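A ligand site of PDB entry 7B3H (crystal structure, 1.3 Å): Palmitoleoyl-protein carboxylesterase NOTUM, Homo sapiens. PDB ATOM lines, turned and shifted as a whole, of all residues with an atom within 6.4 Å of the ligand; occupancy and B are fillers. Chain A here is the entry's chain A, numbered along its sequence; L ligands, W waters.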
ATOM      1  N   GLY A  49     -17.153  -6.183   8.287  1.00  0.00           N
ATOM      2  CA  GLY A  49     -16.808  -6.304   6.885  1.00  0.00           C
ATOM      3  C   GLY A  49     -18.032  -6.365   5.985  1.00  0.00           C
ATOM      4  O   GLY A  49     -19.156  -6.068   6.393  1.00  0.00           O
ATOM      5  N   GLY A  50     -17.776  -6.729   4.721  1.00  0.00           N
ATOM      6  CA  GLY A  50     -18.825  -6.827   3.717  1.00  0.00           C
ATOM      7  C   GLY A  50     -18.477  -6.229   2.362  1.00  0.00           C
ATOM      8  O   GLY A  50     -19.280  -5.506   1.771  1.00  0.00           O
ATOM      9  N   TRP A  51     -17.291  -6.536   1.836  1.00  0.00           N
ATOM     10  CA  TRP A  51     -16.861  -6.149   0.470  1.00  0.00           C
ATOM     11  C   TRP A  51     -16.903  -4.627   0.370  1.00  0.00           C
ATOM     12  O   TRP A  51     -16.451  -3.941   1.303  1.00  0.00           O
ATOM     13  CB  TRP A  51     -17.628  -6.927  -0.576  1.00  0.00           C
ATOM     14  CG  TRP A  51     -17.236  -8.349  -0.569  1.00  0.00           C
ATOM     15  CD1 TRP A  51     -17.907  -9.370   0.017  1.00  0.00           C
ATOM     16  CD2 TRP A  51     -16.103  -8.929  -1.223  1.00  0.00           C
ATOM     17  NE1 TRP A  51     -17.251 -10.564  -0.206  1.00  0.00           N
ATOM     18  CE2 TRP A  51     -16.135 -10.311  -0.965  1.00  0.00           C
ATOM     19  CE3 TRP A  51     -15.053  -8.408  -1.982  1.00  0.00           C
ATOM     20  CZ2 TRP A  51     -15.166 -11.198  -1.459  1.00  0.00           C
ATOM     21  CZ3 TRP A  51     -14.083  -9.282  -2.477  1.00  0.00           C
ATOM     22  CH2 TRP A  51     -14.157 -10.661  -2.205  1.00  0.00           C
ATOM     23  N   TYR A  52     -17.407  -4.069  -0.733  1.00  0.00           N
ATOM     24  CA  TYR A  52     -17.345  -2.648  -1.033  1.00  0.00           C
ATOM     25  C   TYR A  52     -18.103  -2.432  -2.331  1.00  0.00           C
ATOM     26  O   TYR A  52     -18.539  -3.408  -2.955  1.00  0.00           O
ATOM     27  CB  TYR A  52     -15.901  -2.164  -1.176  1.00  0.00           C
ATOM     28  CG  TYR A  52     -15.104  -2.836  -2.258  1.00  0.00           C
ATOM     29  CD1 TYR A  52     -15.078  -2.321  -3.547  1.00  0.00           C
ATOM     30  CD2 TYR A  52     -14.369  -3.983  -1.993  1.00  0.00           C
ATOM     31  CE1 TYR A  52     -14.364  -2.928  -4.557  1.00  0.00           C
ATOM     32  CE2 TYR A  52     -13.632  -4.612  -3.004  1.00  0.00           C
ATOM     33  CZ  TYR A  52     -13.636  -4.073  -4.276  1.00  0.00           C
ATOM     34  OH  TYR A  52     -12.900  -4.680  -5.276  1.00  0.00           O
ATOM     35  N   TYR A 105     -20.425  -1.386   9.307  1.00  0.00           N
ATOM     36  CA  TYR A 105     -19.817  -0.992   8.045  1.00  0.00           C
ATOM     37  C   TYR A 105     -20.925  -0.486   7.126  1.00  0.00           C
ATOM     38  O   TYR A 105     -21.725  -1.270   6.623  1.00  0.00           O
ATOM     39  CB  TYR A 105     -19.150  -2.220   7.455  1.00  0.00           C
ATOM     40  CG  TYR A 105     -18.442  -2.046   6.148  1.00  0.00           C
ATOM     41  CD1 TYR A 105     -17.674  -0.917   5.875  1.00  0.00           C
ATOM     42  CD2 TYR A 105     -18.475  -3.057   5.192  1.00  0.00           C
ATOM     43  CE1 TYR A 105     -16.977  -0.787   4.680  1.00  0.00           C
ATOM     44  CE2 TYR A 105     -17.774  -2.941   4.007  1.00  0.00           C
ATOM     45  CZ  TYR A 105     -17.037  -1.816   3.752  1.00  0.00           C
ATOM     46  OH  TYR A 105     -16.348  -1.720   2.562  1.00  0.00           O
ATOM     47  N   VAL A 110     -14.081  -0.035   2.228  1.00  0.00           N
ATOM     48  CA  VAL A 110     -13.078  -0.806   2.968  1.00  0.00           C
ATOM     49  C   VAL A 110     -12.516   0.115   4.065  1.00  0.00           C
ATOM     50  O   VAL A 110     -11.324   0.066   4.428  1.00  0.00           O
ATOM     51  CB  VAL A 110     -11.982  -1.341   2.022  1.00  0.00           C
ATOM     52  CG1 VAL A 110     -11.006  -2.273   2.757  1.00  0.00           C
ATOM     53  CG2 VAL A 110     -12.562  -1.963   0.781  1.00  0.00           C
ATOM     54  N   SER A 154     -13.004  -7.773  10.763  1.00  0.00           N
ATOM     55  CA  SER A 154     -13.014  -8.984   9.948  1.00  0.00           C
ATOM     56  C   SER A 154     -13.305  -8.649   8.499  1.00  0.00           C
ATOM     57  O   SER A 154     -14.167  -7.808   8.209  1.00  0.00           O
ATOM     58  CB  SER A 154     -14.058  -9.987  10.430  1.00  0.00           C
ATOM     59  OG  SER A 154     -13.769 -10.450  11.741  1.00  0.00           O
ATOM     60  N   SER A 155     -12.593  -9.328   7.596  1.00  0.00           N
ATOM     61  CA  SER A 155     -12.810  -9.225   6.142  1.00  0.00           C
ATOM     62  C   SER A 155     -12.475  -7.808   5.680  1.00  0.00           C
ATOM     63  O   SER A 155     -11.359  -7.340   5.930  1.00  0.00           O
ATOM     64  CB  SER A 155     -14.199  -9.703   5.752  1.00  0.00           C
ATOM     65  OG  SER A 155     -14.434 -11.003   6.269  1.00  0.00           O
ATOM     66  N   ALA A 156     -13.400  -7.102   5.010  1.00  0.00           N
ATOM     67  CA  ALA A 156     -13.136  -5.701   4.707  1.00  0.00           C
ATOM     68  C   ALA A 156     -12.792  -4.915   5.958  1.00  0.00           C
ATOM     69  O   ALA A 156     -12.006  -3.967   5.898  1.00  0.00           O
ATOM     70  CB  ALA A 156     -14.321  -5.068   3.973  1.00  0.00           C
ATOM     71  N   GLY A 157     -13.350  -5.304   7.109  1.00  0.00           N
ATOM     72  CA  GLY A 157     -12.986  -4.667   8.374  1.00  0.00           C
ATOM     73  C   GLY A 157     -11.574  -4.988   8.830  1.00  0.00           C
ATOM     74  O   GLY A 157     -10.923  -4.166   9.480  1.00  0.00           O
ATOM     75  N   THR A 159      -8.982  -5.536   6.681  1.00  0.00           N
ATOM     76  CA  THR A 159      -8.195  -4.582   5.898  1.00  0.00           C
ATOM     77  C   THR A 159      -8.355  -3.175   6.452  1.00  0.00           C
ATOM     78  O   THR A 159      -7.388  -2.394   6.542  1.00  0.00           O
ATOM     79  CB  THR A 159      -8.611  -4.630   4.425  1.00  0.00           C
ATOM     80  OG1 THR A 159      -8.604  -6.001   3.984  1.00  0.00           O
ATOM     81  CG2 THR A 159      -7.686  -3.803   3.561  1.00  0.00           C
ATOM     82  N   SER A 188      -8.880 -11.964   8.624  1.00  0.00           N
ATOM     83  CA  SER A 188      -9.393 -12.275   7.293  1.00  0.00           C
ATOM     84  C   SER A 188      -9.344 -11.077   6.352  1.00  0.00           C
ATOM     85  O   SER A 188     -10.179 -10.951   5.439  1.00  0.00           O
ATOM     86  CB  SER A 188     -10.793 -12.886   7.377  1.00  0.00           C
ATOM     87  OG  SER A 188     -10.743 -14.053   8.200  1.00  0.00           O
ATOM     88  N   GLY A 189      -8.358 -10.200   6.557  1.00  0.00           N
ATOM     89  CA  GLY A 189      -8.193  -9.039   5.723  1.00  0.00           C
ATOM     90  C   GLY A 189      -6.844  -8.960   5.037  1.00  0.00           C
ATOM     91  O   GLY A 189      -6.462  -7.880   4.552  1.00  0.00           O
ATOM     92  N   PHE A 191      -4.809 -10.244   2.077  1.00  0.00           N
ATOM     93  CA  PHE A 191      -5.011 -10.851   0.774  1.00  0.00           C
ATOM     94  C   PHE A 191      -3.753 -10.767  -0.080  1.00  0.00           C
ATOM     95  O   PHE A 191      -2.876  -9.931   0.156  1.00  0.00           O
ATOM     96  CB  PHE A 191      -6.170 -10.162   0.046  1.00  0.00           C
ATOM     97  CG  PHE A 191      -7.456 -10.293   0.777  1.00  0.00           C
ATOM     98  CD1 PHE A 191      -8.082 -11.511   0.885  1.00  0.00           C
ATOM     99  CD2 PHE A 191      -7.993  -9.203   1.454  1.00  0.00           C
ATOM    100  CE1 PHE A 191      -9.241 -11.642   1.622  1.00  0.00           C
ATOM    101  CE2 PHE A 191      -9.149  -9.322   2.165  1.00  0.00           C
ATOM    102  CZ  PHE A 191      -9.772 -10.519   2.261  1.00  0.00           C
ATOM    103  N   LEU A 192      -3.697 -11.623  -1.090  1.00  0.00           N
ATOM    104  CA  LEU A 192      -2.608 -11.605  -2.052  1.00  0.00           C
ATOM    105  C   LEU A 192      -3.109 -11.138  -3.400  1.00  0.00           C
ATOM    106  O   LEU A 192      -4.180 -11.548  -3.864  1.00  0.00           O
ATOM    107  CB  LEU A 192      -2.020 -13.013  -2.231  1.00  0.00           C
ATOM    108  CG  LEU A 192      -1.555 -13.709  -0.963  1.00  0.00           C
ATOM    109  CD1 LEU A 192      -1.068 -15.099  -1.327  1.00  0.00           C
ATOM    110  CD2 LEU A 192      -0.469 -12.912  -0.269  1.00  0.00           C
ATOM    111  N   ASP A 193      -2.327 -10.254  -4.028  1.00  0.00           N
ATOM    112  CA  ASP A 193      -2.584  -9.832  -5.404  1.00  0.00           C
ATOM    113  C   ASP A 193      -1.906 -10.796  -6.376  1.00  0.00           C
ATOM    114  O   ASP A 193      -1.027 -10.437  -7.148  1.00  0.00           O
ATOM    115  CB  ASP A 193      -2.162  -8.387  -5.628  1.00  0.00           C
ATOM    116  CG  ASP A 193      -0.722  -8.092  -5.150  1.00  0.00           C
ATOM    117  OD1 ASP A 193      -0.115  -8.880  -4.406  1.00  0.00           O
ATOM    118  OD2 ASP A 193      -0.186  -7.039  -5.551  1.00  0.00           O
ATOM    119  N   PRO A 210     -11.215  -7.519  -8.124  1.00  0.00           N
ATOM    120  CA  PRO A 210      -9.773  -7.634  -8.316  1.00  0.00           C
ATOM    121  C   PRO A 210      -9.053  -6.348  -7.958  1.00  0.00           C
ATOM    122  O   PRO A 210      -9.635  -5.511  -7.263  1.00  0.00           O
ATOM    123  CB  PRO A 210      -9.633  -7.931  -9.815  1.00  0.00           C
ATOM    124  CG  PRO A 210     -11.005  -8.370 -10.238  1.00  0.00           C
ATOM    125  CD  PRO A 210     -11.916  -7.526  -9.417  1.00  0.00           C
ATOM    126  N   THR A 211      -7.796  -6.194  -8.393  1.00  0.00           N
ATOM    127  CA  THR A 211      -7.062  -4.982  -8.054  1.00  0.00           C
ATOM    128  C   THR A 211      -7.602  -3.788  -8.831  1.00  0.00           C
ATOM    129  O   THR A 211      -7.535  -2.661  -8.339  1.00  0.00           O
ATOM    130  CB  THR A 211      -5.571  -5.126  -8.368  1.00  0.00           C
ATOM    131  OG1 THR A 211      -5.404  -5.616  -9.706  1.00  0.00           O
ATOM    132  CG2 THR A 211      -4.924  -6.111  -7.401  1.00  0.00           C
ATOM    133  N   ILE A 214     -10.469  -2.293  -6.821  1.00  0.00           N
ATOM    134  CA  ILE A 214      -9.978  -1.473  -5.705  1.00  0.00           C
ATOM    135  C   ILE A 214      -9.418  -0.158  -6.217  1.00  0.00           C
ATOM    136  O   ILE A 214      -9.635   0.906  -5.637  1.00  0.00           O
ATOM    137  CB  ILE A 214      -8.943  -2.256  -4.879  1.00  0.00           C
ATOM    138  CG1 ILE A 214      -9.624  -3.372  -4.087  1.00  0.00           C
ATOM    139  CG2 ILE A 214      -8.168  -1.307  -3.944  1.00  0.00           C
ATOM    140  CD1 ILE A 214     -10.536  -2.855  -2.994  1.00  0.00           C
ATOM    141  N   PHE A 242      -3.727  -1.661   0.181  1.00  0.00           N
ATOM    142  CA  PHE A 242      -4.833  -2.521   0.593  1.00  0.00           C
ATOM    143  C   PHE A 242      -4.392  -3.966   0.769  1.00  0.00           C
ATOM    144  O   PHE A 242      -5.195  -4.795   1.199  1.00  0.00           O
ATOM    145  CB  PHE A 242      -5.969  -2.452  -0.431  1.00  0.00           C
ATOM    146  CG  PHE A 242      -6.856  -1.247  -0.292  1.00  0.00           C
ATOM    147  CD1 PHE A 242      -6.336   0.037  -0.339  1.00  0.00           C
ATOM    148  CD2 PHE A 242      -8.228  -1.402  -0.149  1.00  0.00           C
ATOM    149  CE1 PHE A 242      -7.168   1.145  -0.220  1.00  0.00           C
ATOM    150  CE2 PHE A 242      -9.057  -0.308  -0.021  1.00  0.00           C
ATOM    151  CZ  PHE A 242      -8.533   0.970  -0.046  1.00  0.00           C
ATOM    152  N   PHE A 243      -3.135  -4.275   0.433  1.00  0.00           N
ATOM    153  CA  PHE A 243      -2.626  -5.628   0.544  1.00  0.00           C
ATOM    154  C   PHE A 243      -1.741  -5.735   1.776  1.00  0.00           C
ATOM    155  O   PHE A 243      -0.728  -5.034   1.886  1.00  0.00           O
ATOM    156  CB  PHE A 243      -1.928  -6.028  -0.761  1.00  0.00           C
ATOM    157  CG  PHE A 243      -2.908  -6.249  -1.851  1.00  0.00           C
ATOM    158  CD1 PHE A 243      -3.488  -7.484  -2.025  1.00  0.00           C
ATOM    159  CD2 PHE A 243      -3.370  -5.179  -2.603  1.00  0.00           C
ATOM    160  CE1 PHE A 243      -4.461  -7.691  -2.980  1.00  0.00           C
ATOM    161  CE2 PHE A 243      -4.353  -5.357  -3.552  1.00  0.00           C
ATOM    162  CZ  PHE A 243      -4.899  -6.624  -3.746  1.00  0.00           C
ATOM    163  N   ASP A 263      -8.196 -18.872   2.609  1.00  0.00           N
ATOM    164  CA  ASP A 263      -9.384 -18.064   2.815  1.00  0.00           C
ATOM    165  C   ASP A 263     -10.346 -18.183   1.643  1.00  0.00           C
ATOM    166  O   ASP A 263      -9.947 -18.039   0.486  1.00  0.00           O
ATOM    167  CB  ASP A 263      -8.943 -16.621   3.000  1.00  0.00           C
ATOM    168  CG  ASP A 263     -10.056 -15.728   3.417  1.00  0.00           C
ATOM    169  OD1 ASP A 263     -10.668 -15.191   2.482  1.00  0.00           O
ATOM    170  OD2 ASP A 263     -10.306 -15.553   4.610  1.00  0.00           O
ATOM    171  N   ALA A 265     -12.588 -16.152   0.576  1.00  0.00           N
ATOM    172  CA  ALA A 265     -12.683 -14.953  -0.244  1.00  0.00           C
ATOM    173  C   ALA A 265     -11.468 -14.799  -1.154  1.00  0.00           C
ATOM    174  O   ALA A 265     -11.609 -14.337  -2.298  1.00  0.00           O
ATOM    175  CB  ALA A 265     -12.862 -13.713   0.637  1.00  0.00           C
ATOM    176  N   GLN A 266     -10.282 -15.190  -0.679  1.00  0.00           N
ATOM    177  CA  GLN A 266      -9.112 -15.222  -1.537  1.00  0.00           C
ATOM    178  C   GLN A 266      -9.350 -16.174  -2.708  1.00  0.00           C
ATOM    179  O   GLN A 266      -9.085 -15.838  -3.871  1.00  0.00           O
ATOM    180  CB  GLN A 266      -7.886 -15.670  -0.735  1.00  0.00           C
ATOM    181  CG  GLN A 266      -6.613 -15.784  -1.560  1.00  0.00           C
ATOM    182  CD  GLN A 266      -5.994 -14.429  -1.910  1.00  0.00           C
ATOM    183  OE1 GLN A 266      -5.784 -13.582  -1.034  1.00  0.00           O
ATOM    184  NE2 GLN A 266      -5.697 -14.214  -3.195  1.00  0.00           N
ATOM    185  N   VAL A 269     -11.796 -14.539  -5.267  1.00  0.00           N
ATOM    186  CA  VAL A 269     -11.161 -13.589  -6.180  1.00  0.00           C
ATOM    187  C   VAL A 269     -10.191 -14.286  -7.120  1.00  0.00           C
ATOM    188  O   VAL A 269      -9.898 -13.778  -8.207  1.00  0.00           O
ATOM    189  CB  VAL A 269     -10.535 -12.386  -5.451  1.00  0.00           C
ATOM    190  CG1 VAL A 269     -11.581 -11.647  -4.619  1.00  0.00           C
ATOM    191  CG2 VAL A 269      -9.340 -12.787  -4.597  1.00  0.00           C
HETATM  192  C1  LIG L   1      -8.419  -8.316  -3.563  1.00  0.00           C
HETATM  193  C2  LIG L   1      -8.843  -6.558  -2.008  1.00  0.00           C
HETATM  194  C3  LIG L   1      -7.814  -6.280  -1.122  1.00  0.00           C
HETATM  195  C4  LIG L   1      -8.091  -5.913   0.189  1.00  0.00           C
HETATM  196  C5  LIG L   1      -9.392  -5.801   0.635  1.00  0.00           C
HETATM  197  C6  LIG L   1     -10.425  -6.065  -0.260  1.00  0.00           C
HETATM  198  C7  LIG L   1     -10.161  -6.446  -1.564  1.00  0.00           C
HETATM  199  C8  LIG L   1     -12.674  -7.586   0.677  1.00  0.00           C
HETATM  200  C9  LIG L   1     -15.262  -9.179   2.736  1.00  0.00           C
HETATM  201  C10 LIG L   1     -13.653 -10.051   1.373  1.00  0.00           C
HETATM  202  C11 LIG L   1     -12.579  -9.986   0.489  1.00  0.00           C
HETATM  203  C12 LIG L   1     -12.070  -8.745   0.124  1.00  0.00           C
HETATM  204  F1  LIG L   1      -7.668  -8.866  -2.571  1.00  0.00           F
HETATM  205  F2  LIG L   1      -7.859  -8.484  -4.789  1.00  0.00           F
HETATM  206  F3  LIG L   1      -9.636  -8.918  -3.518  1.00  0.00           F
HETATM  207  N1  LIG L   1     -13.687  -7.665   1.513  1.00  0.00           N
HETATM  208  N2  LIG L   1     -14.176  -8.894   1.854  1.00  0.00           N
HETATM  209  N3  LIG L   1     -15.425 -10.584   2.793  1.00  0.00           N
HETATM  210  N4  LIG L   1     -14.452 -11.148   1.978  1.00  0.00           N
HETATM  211  O1  LIG L   1      -8.565  -6.941  -3.343  1.00  0.00           O
HETATM  212  O2  LIG L   1     -15.858  -8.331   3.323  1.00  0.00           O
HETATM  213  S1  LIG L   1     -12.145  -5.908   0.306  1.00  0.00           S
HETATM  214  O   HOH W   1     -11.684  -6.921  -5.003  1.00  0.00           O
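C of Gly 49 touches O2 of the ligand, at 3.96 Å.
CD2 of Tyr 52 touches S1 of the ligand, at 3.7 Å.
CG2 of Val 110 touches S1 of the ligand, at 3.995 Å.
Ser 155 touches the ligand.
Thr 159 touches the ligand.
CB of Phe 191 touches F1 of the ligand (3.3 Å).
CG1 of Ile 214 touches O1 of the ligand, 3.8 Å away.
Phe 242 touches the ligand.
CE1 of Phe 243 touches F1 of the ligand, at 3.4 Å.
Ala 265 touches the ligand (CB to N4, 3.3 Å).
CG1 of Val 269 touches F3 of the ligand, at 3.5 Å.
Hydrophobic or aromatic side chains that line the ligand: Trp 51, Tyr 52, Val 110, Ala 156, Phe 191, Ile 214, Phe 243, Ala 265 and Val 269.
Of the 25 residues printed, 14 come within 4 Å of the ligand.
The side-chain hydroxyl (OH) of Tyr 105 lies within hydrogen-bond range of the backbone carbonyl oxygen (O) of Trp 51 (2.6 Å).
The backbone NH of Ala 265 sits at hydrogen-bond distance from the side-chain carboxylate of Asp 263.
O of Gly 189 sits at hydrogen-bond distance from OG1 of Thr 159, 2.9 Å away.
N of Gly 49 lies close to O of Ser 154, 3.4 Å away.
OH of Tyr 105 sits at hydrogen-bond distance from N of Val 110.
Water W1 bridges the side-chain hydroxyl of Tyr 52 and the backbone carbonyl oxygen of Pro 210.
The backbone NH (N) of Trp 51 sits at hydrogen-bond distance from an oxygen (O2) of the ligand.
The backbone NH of Gly 50 lies within hydrogen-bond range of an oxygen (O2) of the ligand (2.9 Å).
The backbone NH (N) of Ala 156 sits at hydrogen-bond distance from an oxygen (O2) of the ligand (3.2 Å).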
